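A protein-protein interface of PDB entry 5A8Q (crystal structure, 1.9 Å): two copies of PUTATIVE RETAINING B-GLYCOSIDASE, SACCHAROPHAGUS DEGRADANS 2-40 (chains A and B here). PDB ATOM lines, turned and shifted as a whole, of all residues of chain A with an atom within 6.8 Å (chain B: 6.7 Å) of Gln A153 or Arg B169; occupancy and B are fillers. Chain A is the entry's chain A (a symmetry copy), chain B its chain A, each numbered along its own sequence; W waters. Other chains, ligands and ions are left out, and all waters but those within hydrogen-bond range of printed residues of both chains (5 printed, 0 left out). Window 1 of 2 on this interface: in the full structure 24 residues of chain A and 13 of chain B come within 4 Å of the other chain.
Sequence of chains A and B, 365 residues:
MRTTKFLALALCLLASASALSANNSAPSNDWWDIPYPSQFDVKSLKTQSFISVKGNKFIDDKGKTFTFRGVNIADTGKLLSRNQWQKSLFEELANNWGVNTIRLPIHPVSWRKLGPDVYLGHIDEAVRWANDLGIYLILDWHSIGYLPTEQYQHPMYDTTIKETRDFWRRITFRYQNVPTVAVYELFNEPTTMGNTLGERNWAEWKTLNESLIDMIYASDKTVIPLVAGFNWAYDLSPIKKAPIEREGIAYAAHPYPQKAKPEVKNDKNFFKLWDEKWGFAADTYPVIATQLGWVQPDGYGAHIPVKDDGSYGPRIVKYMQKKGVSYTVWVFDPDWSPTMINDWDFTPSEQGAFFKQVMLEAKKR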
ATOM      1  N   SER A 143      24.506  -1.162   9.828  1.00  0.00           N
ATOM      2  CA  SER A 143      23.437  -1.996   9.326  1.00  0.00           C
ATOM      3  C   SER A 143      23.688  -3.464   9.685  1.00  0.00           C
ATOM      4  O   SER A 143      24.808  -3.863  10.070  1.00  0.00           O
ATOM      5  CB  SER A 143      23.315  -1.789   7.804  1.00  0.00           C
ATOM      6  OG  SER A 143      22.254  -2.541   7.262  1.00  0.00           O
ATOM      7  N   ILE A 144      22.624  -4.252   9.605  1.00  0.00           N
ATOM      8  CA  ILE A 144      22.664  -5.686   9.815  1.00  0.00           C
ATOM      9  C   ILE A 144      21.860  -6.327   8.687  1.00  0.00           C
ATOM     10  O   ILE A 144      20.668  -6.071   8.544  1.00  0.00           O
ATOM     11  CB  ILE A 144      22.030  -6.127  11.159  1.00  0.00           C
ATOM     12  CG1 ILE A 144      22.619  -5.356  12.349  1.00  0.00           C
ATOM     13  CG2 ILE A 144      22.223  -7.621  11.338  1.00  0.00           C
ATOM     14  CD1 ILE A 144      22.208  -5.874  13.719  1.00  0.00           C
ATOM     15  N   GLY A 145      22.517  -7.153   7.887  1.00  0.00           N
ATOM     16  CA  GLY A 145      21.850  -7.837   6.810  1.00  0.00           C
ATOM     17  C   GLY A 145      22.772  -8.085   5.648  1.00  0.00           C
ATOM     18  O   GLY A 145      23.988  -8.171   5.813  1.00  0.00           O
ATOM     19  N   TYR A 146      22.175  -8.211   4.465  1.00  0.00           N
ATOM     20  CA  TYR A 146      22.910  -8.586   3.269  1.00  0.00           C
ATOM     21  C   TYR A 146      22.772  -7.493   2.215  1.00  0.00           C
ATOM     22  O   TYR A 146      21.759  -7.381   1.523  1.00  0.00           O
ATOM     23  CB  TYR A 146      22.431  -9.938   2.733  1.00  0.00           C
ATOM     24  CG  TYR A 146      23.456 -10.589   1.819  1.00  0.00           C
ATOM     25  CD1 TYR A 146      24.743 -10.851   2.273  1.00  0.00           C
ATOM     26  CD2 TYR A 146      23.142 -10.931   0.507  1.00  0.00           C
ATOM     27  CE1 TYR A 146      25.696 -11.430   1.441  1.00  0.00           C
ATOM     28  CE2 TYR A 146      24.081 -11.519  -0.323  1.00  0.00           C
ATOM     29  CZ  TYR A 146      25.357 -11.763   0.148  1.00  0.00           C
ATOM     30  OH  TYR A 146      26.295 -12.337  -0.675  1.00  0.00           O
ATOM     31  N   GLN A 151      18.500  -6.561   1.751  1.00  0.00           N
ATOM     32  CA  GLN A 151      17.565  -7.111   2.724  1.00  0.00           C
ATOM     33  C   GLN A 151      18.231  -7.146   4.099  1.00  0.00           C
ATOM     34  O   GLN A 151      19.399  -7.518   4.215  1.00  0.00           O
ATOM     35  CB  GLN A 151      17.139  -8.527   2.324  1.00  0.00           C
ATOM     36  CG  GLN A 151      16.632  -8.684   0.911  1.00  0.00           C
ATOM     37  CD  GLN A 151      15.322  -7.956   0.657  1.00  0.00           C
ATOM     38  OE1 GLN A 151      14.285  -8.269   1.268  1.00  0.00           O
ATOM     39  NE2 GLN A 151      15.351  -6.996  -0.256  1.00  0.00           N
ATOM     40  N   TYR A 152      17.469  -6.809   5.146  1.00  0.00           N
ATOM     41  CA  TYR A 152      18.042  -6.523   6.464  1.00  0.00           C
ATOM     42  C   TYR A 152      17.295  -7.176   7.620  1.00  0.00           C
ATOM     43  O   TYR A 152      16.160  -7.642   7.491  1.00  0.00           O
ATOM     44  CB  TYR A 152      18.130  -4.996   6.679  1.00  0.00           C
ATOM     45  CG  TYR A 152      18.821  -4.352   5.509  1.00  0.00           C
ATOM     46  CD1 TYR A 152      20.209  -4.354   5.410  1.00  0.00           C
ATOM     47  CD2 TYR A 152      18.081  -3.873   4.437  1.00  0.00           C
ATOM     48  CE1 TYR A 152      20.841  -3.831   4.297  1.00  0.00           C
ATOM     49  CE2 TYR A 152      18.702  -3.340   3.331  1.00  0.00           C
ATOM     50  CZ  TYR A 152      20.084  -3.329   3.262  1.00  0.00           C
ATOM     51  OH  TYR A 152      20.706  -2.807   2.151  1.00  0.00           O
ATOM     52  N   GLN A 153      17.954  -7.209   8.769  1.00  0.00           N
ATOM     53  CA  GLN A 153      17.358  -7.812   9.956  1.00  0.00           C
ATOM     54  C   GLN A 153      16.167  -7.009  10.510  1.00  0.00           C
ATOM     55  O   GLN A 153      15.265  -7.583  11.122  1.00  0.00           O
ATOM     56  CB  GLN A 153      18.431  -7.977  11.038  1.00  0.00           C
ATOM     57  CG  GLN A 153      17.907  -8.529  12.352  1.00  0.00           C
ATOM     58  CD  GLN A 153      19.009  -9.091  13.237  1.00  0.00           C
ATOM     59  OE1 GLN A 153      19.887  -9.784  12.773  1.00  0.00           O
ATOM     60  NE2 GLN A 153      18.949  -8.799  14.521  1.00  0.00           N
ATOM     61  N   HIS A 154      16.188  -5.688  10.327  1.00  0.00           N
ATOM     62  CA  HIS A 154      15.199  -4.779  10.926  1.00  0.00           C
ATOM     63  C   HIS A 154      15.234  -3.460  10.144  1.00  0.00           C
ATOM     64  O   HIS A 154      16.297  -3.073   9.662  1.00  0.00           O
ATOM     65  CB  HIS A 154      15.563  -4.544  12.389  1.00  0.00           C
ATOM     66  CG  HIS A 154      14.570  -3.739  13.170  1.00  0.00           C
ATOM     67  ND1 HIS A 154      14.469  -2.370  13.059  1.00  0.00           N
ATOM     68  CD2 HIS A 154      13.675  -4.103  14.123  1.00  0.00           C
ATOM     69  CE1 HIS A 154      13.541  -1.923  13.886  1.00  0.00           C
ATOM     70  NE2 HIS A 154      13.045  -2.956  14.548  1.00  0.00           N
ATOM     71  N   PRO A 155      14.079  -2.776  10.003  1.00  0.00           N
ATOM     72  CA  PRO A 155      14.051  -1.520   9.231  1.00  0.00           C
ATOM     73  C   PRO A 155      14.971  -0.394   9.722  1.00  0.00           C
ATOM     74  O   PRO A 155      15.352   0.432   8.917  1.00  0.00           O
ATOM     75  CB  PRO A 155      12.574  -1.072   9.303  1.00  0.00           C
ATOM     76  CG  PRO A 155      11.987  -1.876  10.423  1.00  0.00           C
ATOM     77  CD  PRO A 155      12.716  -3.184  10.392  1.00  0.00           C
ATOM     78  N   MET A 156      15.361  -0.373  10.993  1.00  0.00           N
ATOM     79  CA  MET A 156      16.302   0.624  11.474  1.00  0.00           C
ATOM     80  C   MET A 156      17.645   0.522  10.733  1.00  0.00           C
ATOM     81  O   MET A 156      18.385   1.512  10.637  1.00  0.00           O
ATOM     82  CB  MET A 156      16.496   0.547  13.000  1.00  0.00           C
ATOM     83  CG  MET A 156      17.409  -0.566  13.491  1.00  0.00           C
ATOM     84  SD  MET A 156      17.726  -0.530  15.270  1.00  0.00           S
ATOM     85  CE  MET A 156      16.341  -1.476  15.892  1.00  0.00           C
ATOM     86  N   TYR A 157      17.934  -0.667  10.193  1.00  0.00           N
ATOM     87  CA  TYR A 157      19.158  -0.937   9.443  1.00  0.00           C
ATOM     88  C   TYR A 157      19.018  -0.809   7.912  1.00  0.00           C
ATOM     89  O   TYR A 157      19.996  -1.004   7.187  1.00  0.00           O
ATOM     90  CB  TYR A 157      19.654  -2.347   9.756  1.00  0.00           C
ATOM     91  CG  TYR A 157      19.787  -2.659  11.239  1.00  0.00           C
ATOM     92  CD1 TYR A 157      20.593  -1.890  12.070  1.00  0.00           C
ATOM     93  CD2 TYR A 157      19.074  -3.707  11.810  1.00  0.00           C
ATOM     94  CE1 TYR A 157      20.706  -2.170  13.431  1.00  0.00           C
ATOM     95  CE2 TYR A 157      19.175  -3.990  13.168  1.00  0.00           C
ATOM     96  CZ  TYR A 157      19.983  -3.220  13.974  1.00  0.00           C
ATOM     97  OH  TYR A 157      20.065  -3.528  15.333  1.00  0.00           O
ATOM     98  N   GLU A 189      27.332  -5.489  10.394  1.00  0.00           N
ATOM     99  CA  GLU A 189      27.140  -6.933  10.570  1.00  0.00           C
ATOM    100  C   GLU A 189      26.516  -7.603   9.345  1.00  0.00           C
ATOM    101  O   GLU A 189      25.273  -7.682   9.226  1.00  0.00           O
ATOM    102  CB  GLU A 189      26.329  -7.216  11.842  1.00  0.00           C
ATOM    103  CG  GLU A 189      27.197  -7.136  13.102  1.00  0.00           C
ATOM    104  CD  GLU A 189      26.442  -7.163  14.417  1.00  0.00           C
ATOM    105  OE1 GLU A 189      25.269  -6.775  14.427  1.00  0.00           O
ATOM    106  OE2 GLU A 189      27.061  -7.518  15.469  1.00  0.00           O
ATOM    107  N   THR A 191      25.081 -10.502   7.361  1.00  0.00           N
ATOM    108  CA  THR A 191      24.418 -11.773   7.625  1.00  0.00           C
ATOM    109  C   THR A 191      23.286 -11.968   6.639  1.00  0.00           C
ATOM    110  O   THR A 191      22.692 -10.979   6.183  1.00  0.00           O
ATOM    111  CB  THR A 191      23.850 -11.833   9.065  1.00  0.00           C
ATOM    112  OG1 THR A 191      23.190 -13.083   9.265  1.00  0.00           O
ATOM    113  CG2 THR A 191      22.871 -10.707   9.326  1.00  0.00           C
ATOM    114  N   MET A 193      20.896 -14.261   7.716  1.00  0.00           N
ATOM    115  CA  MET A 193      19.932 -14.898   8.639  1.00  0.00           C
ATOM    116  C   MET A 193      19.482 -16.265   8.132  1.00  0.00           C
ATOM    117  O   MET A 193      18.293 -16.499   7.854  1.00  0.00           O
ATOM    118  CB  MET A 193      18.721 -13.974   8.878  1.00  0.00           C
ATOM    119  CG  MET A 193      19.096 -12.565   9.328  1.00  0.00           C
ATOM    120  SD  MET A 193      17.688 -11.475   9.692  1.00  0.00           S
ATOM    121  CE  MET A 193      17.220 -12.119  11.293  1.00  0.00           C
ATOM    122  N   THR A 196      17.765 -16.487   4.616  1.00  0.00           N
ATOM    123  CA  THR A 196      16.430 -15.906   4.436  1.00  0.00           C
ATOM    124  C   THR A 196      16.497 -14.522   3.768  1.00  0.00           C
ATOM    125  O   THR A 196      15.523 -14.078   3.170  1.00  0.00           O
ATOM    126  CB  THR A 196      15.684 -15.778   5.763  1.00  0.00           C
ATOM    127  OG1 THR A 196      16.443 -14.950   6.667  1.00  0.00           O
ATOM    128  CG2 THR A 196      15.435 -17.170   6.370  1.00  0.00           C
ATOM    129  N   LEU A 197      17.641 -13.849   3.848  1.00  0.00           N
ATOM    130  CA  LEU A 197      17.793 -12.518   3.246  1.00  0.00           C
ATOM    131  C   LEU A 197      18.411 -12.555   1.850  1.00  0.00           C
ATOM    132  O   LEU A 197      18.464 -11.533   1.174  1.00  0.00           O
ATOM    133  CB  LEU A 197      18.658 -11.628   4.130  1.00  0.00           C
ATOM    134  CG  LEU A 197      18.172 -11.417   5.548  1.00  0.00           C
ATOM    135  CD1 LEU A 197      19.122 -10.440   6.242  1.00  0.00           C
ATOM    136  CD2 LEU A 197      16.736 -10.907   5.584  1.00  0.00           C
ATOM    137  N   TRP A 232      26.968 -12.376  11.130  1.00  0.00           N
ATOM    138  CA  TRP A 232      26.998 -11.154  11.935  1.00  0.00           C
ATOM    139  C   TRP A 232      28.434 -10.734  12.302  1.00  0.00           C
ATOM    140  O   TRP A 232      28.746 -10.515  13.467  1.00  0.00           O
ATOM    141  CB  TRP A 232      26.134 -11.292  13.200  1.00  0.00           C
ATOM    142  CG  TRP A 232      24.629 -11.379  12.997  1.00  0.00           C
ATOM    143  CD1 TRP A 232      23.739 -10.358  13.137  1.00  0.00           C
ATOM    144  CD2 TRP A 232      23.843 -12.549  12.679  1.00  0.00           C
ATOM    145  NE1 TRP A 232      22.454 -10.810  12.927  1.00  0.00           N
ATOM    146  CE2 TRP A 232      22.490 -12.145  12.634  1.00  0.00           C
ATOM    147  CE3 TRP A 232      24.148 -13.888  12.428  1.00  0.00           C
ATOM    148  CZ2 TRP A 232      21.447 -13.037  12.361  1.00  0.00           C
ATOM    149  CZ3 TRP A 232      23.114 -14.773  12.151  1.00  0.00           C
ATOM    150  CH2 TRP A 232      21.769 -14.340  12.125  1.00  0.00           C
ATOM    151  N   TYR B  36      10.285  -6.059  16.315  1.00  0.00           N
ATOM    152  CA  TYR B  36      10.502  -7.131  15.365  1.00  0.00           C
ATOM    153  C   TYR B  36       9.158  -7.786  15.044  1.00  0.00           C
ATOM    154  O   TYR B  36       8.267  -7.792  15.879  1.00  0.00           O
ATOM    155  CB  TYR B  36      11.500  -8.158  15.918  1.00  0.00           C
ATOM    156  CG  TYR B  36      12.943  -7.742  15.744  1.00  0.00           C
ATOM    157  CD1 TYR B  36      13.586  -6.955  16.684  1.00  0.00           C
ATOM    158  CD2 TYR B  36      13.671  -8.146  14.625  1.00  0.00           C
ATOM    159  CE1 TYR B  36      14.913  -6.584  16.519  1.00  0.00           C
ATOM    160  CE2 TYR B  36      14.982  -7.781  14.458  1.00  0.00           C
ATOM    161  CZ  TYR B  36      15.606  -7.000  15.394  1.00  0.00           C
ATOM    162  OH  TYR B  36      16.924  -6.625  15.209  1.00  0.00           O
ATOM    163  N   PRO B  37       9.022  -8.351  13.833  1.00  0.00           N
ATOM    164  CA  PRO B  37       7.731  -8.859  13.388  1.00  0.00           C
ATOM    165  C   PRO B  37       7.348 -10.174  14.036  1.00  0.00           C
ATOM    166  O   PRO B  37       8.214 -10.912  14.523  1.00  0.00           O
ATOM    167  CB  PRO B  37       7.943  -9.060  11.885  1.00  0.00           C
ATOM    168  CG  PRO B  37       9.392  -9.363  11.762  1.00  0.00           C
ATOM    169  CD  PRO B  37      10.053  -8.476  12.785  1.00  0.00           C
ATOM    170  N   THR B 164      10.217  -6.420  -3.959  1.00  0.00           N
ATOM    171  CA  THR B 164       9.708  -7.742  -4.266  1.00  0.00           C
ATOM    172  C   THR B 164      10.303  -8.798  -3.313  1.00  0.00           C
ATOM    173  O   THR B 164       9.573  -9.638  -2.767  1.00  0.00           O
ATOM    174  CB  THR B 164       9.974  -8.106  -5.743  1.00  0.00           C
ATOM    175  OG1 THR B 164       9.223  -7.219  -6.589  1.00  0.00           O
ATOM    176  CG2 THR B 164       9.539  -9.533  -6.037  1.00  0.00           C
ATOM    177  N   ARG B 165      11.618  -8.773  -3.124  1.00  0.00           N
ATOM    178  CA  ARG B 165      12.256  -9.664  -2.149  1.00  0.00           C
ATOM    179  C   ARG B 165      11.684  -9.460  -0.758  1.00  0.00           C
ATOM    180  O   ARG B 165      11.421 -10.425  -0.044  1.00  0.00           O
ATOM    181  CB  ARG B 165      13.755  -9.431  -2.087  1.00  0.00           C
ATOM    182  CG  ARG B 165      14.545  -9.862  -3.315  1.00  0.00           C
ATOM    183  CD  ARG B 165      16.028  -9.649  -3.022  1.00  0.00           C
ATOM    184  NE  ARG B 165      16.878  -9.950  -4.155  1.00  0.00           N
ATOM    185  CZ  ARG B 165      17.186 -11.174  -4.555  1.00  0.00           C
ATOM    186  NH1 ARG B 165      16.704 -12.246  -3.918  1.00  0.00           N
ATOM    187  NH2 ARG B 165      17.971 -11.329  -5.613  1.00  0.00           N
ATOM    188  N   ASP B 166      11.506  -8.204  -0.367  1.00  0.00           N
ATOM    189  CA  ASP B 166      11.024  -7.893   0.970  1.00  0.00           C
ATOM    190  C   ASP B 166       9.593  -8.389   1.169  1.00  0.00           C
ATOM    191  O   ASP B 166       9.251  -8.879   2.251  1.00  0.00           O
ATOM    192  CB  ASP B 166      11.109  -6.386   1.255  1.00  0.00           C
ATOM    193  CG  ASP B 166      10.505  -6.029   2.591  1.00  0.00           C
ATOM    194  OD1 ASP B 166      11.117  -6.365   3.631  1.00  0.00           O
ATOM    195  OD2 ASP B 166       9.410  -5.443   2.608  1.00  0.00           O
ATOM    196  N   PHE B 167       8.752  -8.238   0.143  1.00  0.00           N
ATOM    197  CA  PHE B 167       7.394  -8.762   0.208  1.00  0.00           C
ATOM    198  C   PHE B 167       7.449 -10.258   0.489  1.00  0.00           C
ATOM    199  O   PHE B 167       6.823 -10.740   1.435  1.00  0.00           O
ATOM    200  CB  PHE B 167       6.628  -8.467  -1.085  1.00  0.00           C
ATOM    201  CG  PHE B 167       5.293  -9.153  -1.168  1.00  0.00           C
ATOM    202  CD1 PHE B 167       4.193  -8.645  -0.498  1.00  0.00           C
ATOM    203  CD2 PHE B 167       5.143 -10.311  -1.899  1.00  0.00           C
ATOM    204  CE1 PHE B 167       2.957  -9.275  -0.572  1.00  0.00           C
ATOM    205  CE2 PHE B 167       3.914 -10.945  -1.978  1.00  0.00           C
ATOM    206  CZ  PHE B 167       2.822 -10.423  -1.306  1.00  0.00           C
ATOM    207  N   TRP B 168       8.246 -10.997  -0.284  1.00  0.00           N
ATOM    208  CA  TRP B 168       8.299 -12.447  -0.089  1.00  0.00           C
ATOM    209  C   TRP B 168       8.956 -12.828   1.236  1.00  0.00           C
ATOM    210  O   TRP B 168       8.526 -13.795   1.889  1.00  0.00           O
ATOM    211  CB  TRP B 168       8.929 -13.161  -1.308  1.00  0.00           C
ATOM    212  CG  TRP B 168       7.994 -13.130  -2.472  1.00  0.00           C
ATOM    213  CD1 TRP B 168       8.195 -12.520  -3.670  1.00  0.00           C
ATOM    214  CD2 TRP B 168       6.662 -13.653  -2.507  1.00  0.00           C
ATOM    215  NE1 TRP B 168       7.086 -12.650  -4.463  1.00  0.00           N
ATOM    216  CE2 TRP B 168       6.124 -13.337  -3.775  1.00  0.00           C
ATOM    217  CE3 TRP B 168       5.866 -14.343  -1.589  1.00  0.00           C
ATOM    218  CZ2 TRP B 168       4.843 -13.719  -4.156  1.00  0.00           C
ATOM    219  CZ3 TRP B 168       4.591 -14.726  -1.965  1.00  0.00           C
ATOM    220  CH2 TRP B 168       4.085 -14.399  -3.238  1.00  0.00           C
ATOM    221  N   ARG B 169       9.943 -12.049   1.672  1.00  0.00           N
ATOM    222  CA  ARG B 169      10.558 -12.279   2.980  1.00  0.00           C
ATOM    223  C   ARG B 169       9.500 -12.156   4.084  1.00  0.00           C
ATOM    224  O   ARG B 169       9.397 -13.020   4.967  1.00  0.00           O
ATOM    225  CB  ARG B 169      11.725 -11.297   3.196  1.00  0.00           C
ATOM    226  CG  ARG B 169      12.442 -11.402   4.537  1.00  0.00           C
ATOM    227  CD  ARG B 169      11.762 -10.604   5.646  1.00  0.00           C
ATOM    228  NE  ARG B 169      12.553 -10.598   6.888  1.00  0.00           N
ATOM    229  CZ  ARG B 169      13.583  -9.793   7.146  1.00  0.00           C
ATOM    230  NH1 ARG B 169      14.017  -8.909   6.250  1.00  0.00           N
ATOM    231  NH2 ARG B 169      14.202  -9.887   8.321  1.00  0.00           N
ATOM    232  N   ARG B 170       8.720 -11.089   4.041  1.00  0.00           N
ATOM    233  CA  ARG B 170       7.720 -10.838   5.068  1.00  0.00           C
ATOM    234  C   ARG B 170       6.595 -11.875   5.063  1.00  0.00           C
ATOM    235  O   ARG B 170       6.163 -12.349   6.128  1.00  0.00           O
ATOM    236  CB  ARG B 170       7.101  -9.454   4.900  1.00  0.00           C
ATOM    237  CG  ARG B 170       8.009  -8.270   5.183  1.00  0.00           C
ATOM    238  CD  ARG B 170       7.215  -7.025   4.817  1.00  0.00           C
ATOM    239  NE  ARG B 170       7.893  -5.743   4.956  1.00  0.00           N
ATOM    240  CZ  ARG B 170       7.811  -4.918   6.004  1.00  0.00           C
ATOM    241  NH1 ARG B 170       7.143  -5.234   7.109  1.00  0.00           N
ATOM    242  NH2 ARG B 170       8.442  -3.752   5.948  1.00  0.00           N
ATOM    243  N   ILE B 171       6.122 -12.208   3.862  1.00  0.00           N
ATOM    244  CA  ILE B 171       5.051 -13.175   3.689  1.00  0.00           C
ATOM    245  C   ILE B 171       5.478 -14.548   4.198  1.00  0.00           C
ATOM    246  O   ILE B 171       4.736 -15.201   4.929  1.00  0.00           O
ATOM    247  CB  ILE B 171       4.629 -13.268   2.206  1.00  0.00           C
ATOM    248  CG1 ILE B 171       3.910 -11.985   1.772  1.00  0.00           C
ATOM    249  CG2 ILE B 171       3.790 -14.505   1.931  1.00  0.00           C
ATOM    250  CD1 ILE B 171       2.479 -11.846   2.217  1.00  0.00           C
ATOM    251  N   THR B 172       6.671 -14.982   3.822  1.00  0.00           N
ATOM    252  CA  THR B 172       7.100 -16.336   4.137  1.00  0.00           C
ATOM    253  C   THR B 172       7.287 -16.511   5.647  1.00  0.00           C
ATOM    254  O   THR B 172       6.854 -17.519   6.224  1.00  0.00           O
ATOM    255  CB  THR B 172       8.367 -16.731   3.371  1.00  0.00           C
ATOM    256  OG1 THR B 172       8.167 -16.498   1.963  1.00  0.00           O
ATOM    257  CG2 THR B 172       8.654 -18.207   3.586  1.00  0.00           C
ATOM    258  N   PHE B 173       7.893 -15.514   6.284  1.00  0.00           N
ATOM    259  CA  PHE B 173       8.002 -15.486   7.744  1.00  0.00           C
ATOM    260  C   PHE B 173       6.626 -15.507   8.421  1.00  0.00           C
ATOM    261  O   PHE B 173       6.389 -16.311   9.320  1.00  0.00           O
ATOM    262  CB  PHE B 173       8.763 -14.231   8.182  1.00  0.00           C
ATOM    263  CG  PHE B 173       8.889 -14.074   9.673  1.00  0.00           C
ATOM    264  CD1 PHE B 173       9.775 -14.866  10.403  1.00  0.00           C
ATOM    265  CD2 PHE B 173       8.130 -13.131  10.352  1.00  0.00           C
ATOM    266  CE1 PHE B 173       9.894 -14.711  11.774  1.00  0.00           C
ATOM    267  CE2 PHE B 173       8.244 -12.974  11.717  1.00  0.00           C
ATOM    268  CZ  PHE B 173       9.126 -13.761  12.432  1.00  0.00           C
ATOM    269  N   ARG B 174       5.731 -14.610   8.011  1.00  0.00           N
ATOM    270  CA  ARG B 174       4.465 -14.465   8.710  1.00  0.00           C
ATOM    271  C   ARG B 174       3.603 -15.730   8.611  1.00  0.00           C
ATOM    272  O   ARG B 174       2.984 -16.120   9.601  1.00  0.00           O
ATOM    273  CB  ARG B 174       3.664 -13.252   8.230  1.00  0.00           C
ATOM    274  CG  ARG B 174       2.527 -12.881   9.172  1.00  0.00           C
ATOM    275  CD  ARG B 174       1.823 -11.657   8.635  1.00  0.00           C
ATOM    276  NE  ARG B 174       0.780 -11.064   9.473  1.00  0.00           N
ATOM    277  CZ  ARG B 174       0.899  -9.928  10.157  1.00  0.00           C
ATOM    278  NH1 ARG B 174       2.062  -9.278  10.215  1.00  0.00           N
ATOM    279  NH2 ARG B 174      -0.151  -9.437  10.809  1.00  0.00           N
ATOM    280  N   MET B 215      15.192 -17.704  -1.033  1.00  0.00           N
ATOM    281  CA  MET B 215      14.764 -16.920   0.137  1.00  0.00           C
ATOM    282  C   MET B 215      13.554 -17.542   0.814  1.00  0.00           C
ATOM    283  O   MET B 215      13.483 -17.604   2.044  1.00  0.00           O
ATOM    284  CB  MET B 215      14.378 -15.496  -0.257  1.00  0.00           C
ATOM    285  CG  MET B 215      15.515 -14.578  -0.650  1.00  0.00           C
ATOM    286  SD  MET B 215      14.828 -12.959  -1.084  1.00  0.00           S
ATOM    287  CE  MET B 215      14.454 -12.325   0.549  1.00  0.00           C
ATOM    288  N   ILE B 216      12.598 -17.983   0.004  1.00  0.00           N
ATOM    289  CA  ILE B 216      11.356 -18.563   0.507  1.00  0.00           C
ATOM    290  C   ILE B 216      11.629 -19.889   1.201  1.00  0.00           C
ATOM    291  O   ILE B 216      11.246 -20.081   2.373  1.00  0.00           O
ATOM    292  CB  ILE B 216      10.318 -18.715  -0.628  1.00  0.00           C
ATOM    293  CG1 ILE B 216       9.841 -17.331  -1.072  1.00  0.00           C
ATOM    294  CG2 ILE B 216       9.139 -19.557  -0.178  1.00  0.00           C
ATOM    295  CD1 ILE B 216       9.090 -17.296  -2.398  1.00  0.00           C
ATOM    296  N   SER B 219      13.011 -20.064   4.620  1.00  0.00           N
ATOM    297  CA  SER B 219      12.073 -19.602   5.658  1.00  0.00           C
ATOM    298  C   SER B 219      10.901 -20.585   5.861  1.00  0.00           C
ATOM    299  O   SER B 219      10.466 -20.799   6.995  1.00  0.00           O
ATOM    300  CB  SER B 219      11.593 -18.194   5.272  1.00  0.00           C
ATOM    301  OG  SER B 219      10.649 -17.656   6.176  1.00  0.00           O
HETATM  302  O   HOH W   1      13.244  -7.955   3.696  1.00  0.00           O
HETATM  303  O   HOH W   2      18.137  -4.953  16.722  1.00  0.00           O
HETATM  304  O   HOH W   3      14.795  -5.925   4.751  1.00  0.00           O
HETATM  305  O   HOH W   4      12.939 -15.156   3.373  1.00  0.00           O
HETATM  306  O   HOH W   5      12.956  -8.967  11.210  1.00  0.00           O
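Among the printed residues, merely in contact across the chains: Gln A151 with Arg B165 (3.4 Å), Gln A153 with Arg B169 (3.8 Å), His A154 with Tyr B36 (3.7 Å), Thr A196 with Met B215 (3.3 Å) and Leu A197 with Arg B169 (3.4 Å).
The side-chain sulfur (SD) of Met B215 is in hydrogen-bond range of the guanidinium group (NH1) of Arg B165 (3.5 Å).
The backbone carbonyl oxygen (O) of Gln A151 sits at hydrogen-bond distance from the backbone NH (N) of Tyr A146 (2.9 Å).
The guanidinium group (NE) of Arg B170 lies within salt-bridge range of the side-chain carboxylate (OD2) of Asp B166 (2.8 Å).
Of chain B, only Tyr B36 and Arg B169 come within 4 Å of Gln A153.
Of chain A, only Tyr A152, Gln A153 and Leu A197 come within 4 Å of Arg B169.
Printed residues of chain B within 4 Å of Leu A197: Arg B169 (3.4 Å).
Of the printed residues of chain B, Gln A151 touches Arg B165 (3.4 Å) and Asp B166 (3.2 Å).
The nearest printed residue of chain B that does not touch His A154 is Arg B169 (5.1 Å).
Water W2 lies within hydrogen-bond range of OH of Tyr B36 (2.6 Å) and OH of Tyr A157 (2.8 Å).
Water W1 lies within hydrogen-bond range of OD1 of Asp B166, OE1 of Gln A151 and NH1 of Arg B169.
Water W5 bridges the backbone carbonyl oxygen of Gln A153 and the guanidinium group of Arg B169.
Water W4 bridges O of Thr A196 (2.8 Å) and O of Met B215 (2.8 Å).
Water W3 bridges the backbone NH of Tyr A152 (2.8 Å) and the guanidinium group of Arg B169 (3.4 Å).
Of the 17 printed residues of chain A, 6 touch a printed residue of chain B.
Hydrophobic or aromatic side chains of chain A that line the printed part of chain B: His A154 and Leu A197.
Of the 16 printed residues of chain B, 5 touch a printed residue of chain A.
Printed residues of chain B that touch a printed residue of chain A: Tyr B36, Arg B165, Asp B166, Arg B169 and Met B215.
Hydrophobic or aromatic side chains of chain B that line the printed part of chain A: Tyr B36 and Met B215.
Among the printed residues, no Asp or Glu carboxylate lies within 4 Å of a Lys or Arg side-chain nitrogen of the other chain.
No position is printed for both chains.
Of the 8 pairs that touch across the chains among the printed residues, none has its exchanged pair printed and touching as well.
N of Asp B166 lies within hydrogen-bond range of OE1 of Gln A151, at 3.2 Å.
O of Tyr A152 sits at hydrogen-bond distance from NH1 of Arg B169 (2.8 Å).
The side-chain hydroxyl (OH) of Tyr B36 lies within hydrogen-bond range of the side-chain amide nitrogen (NE2) of Gln A153, 3.0 Å away.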
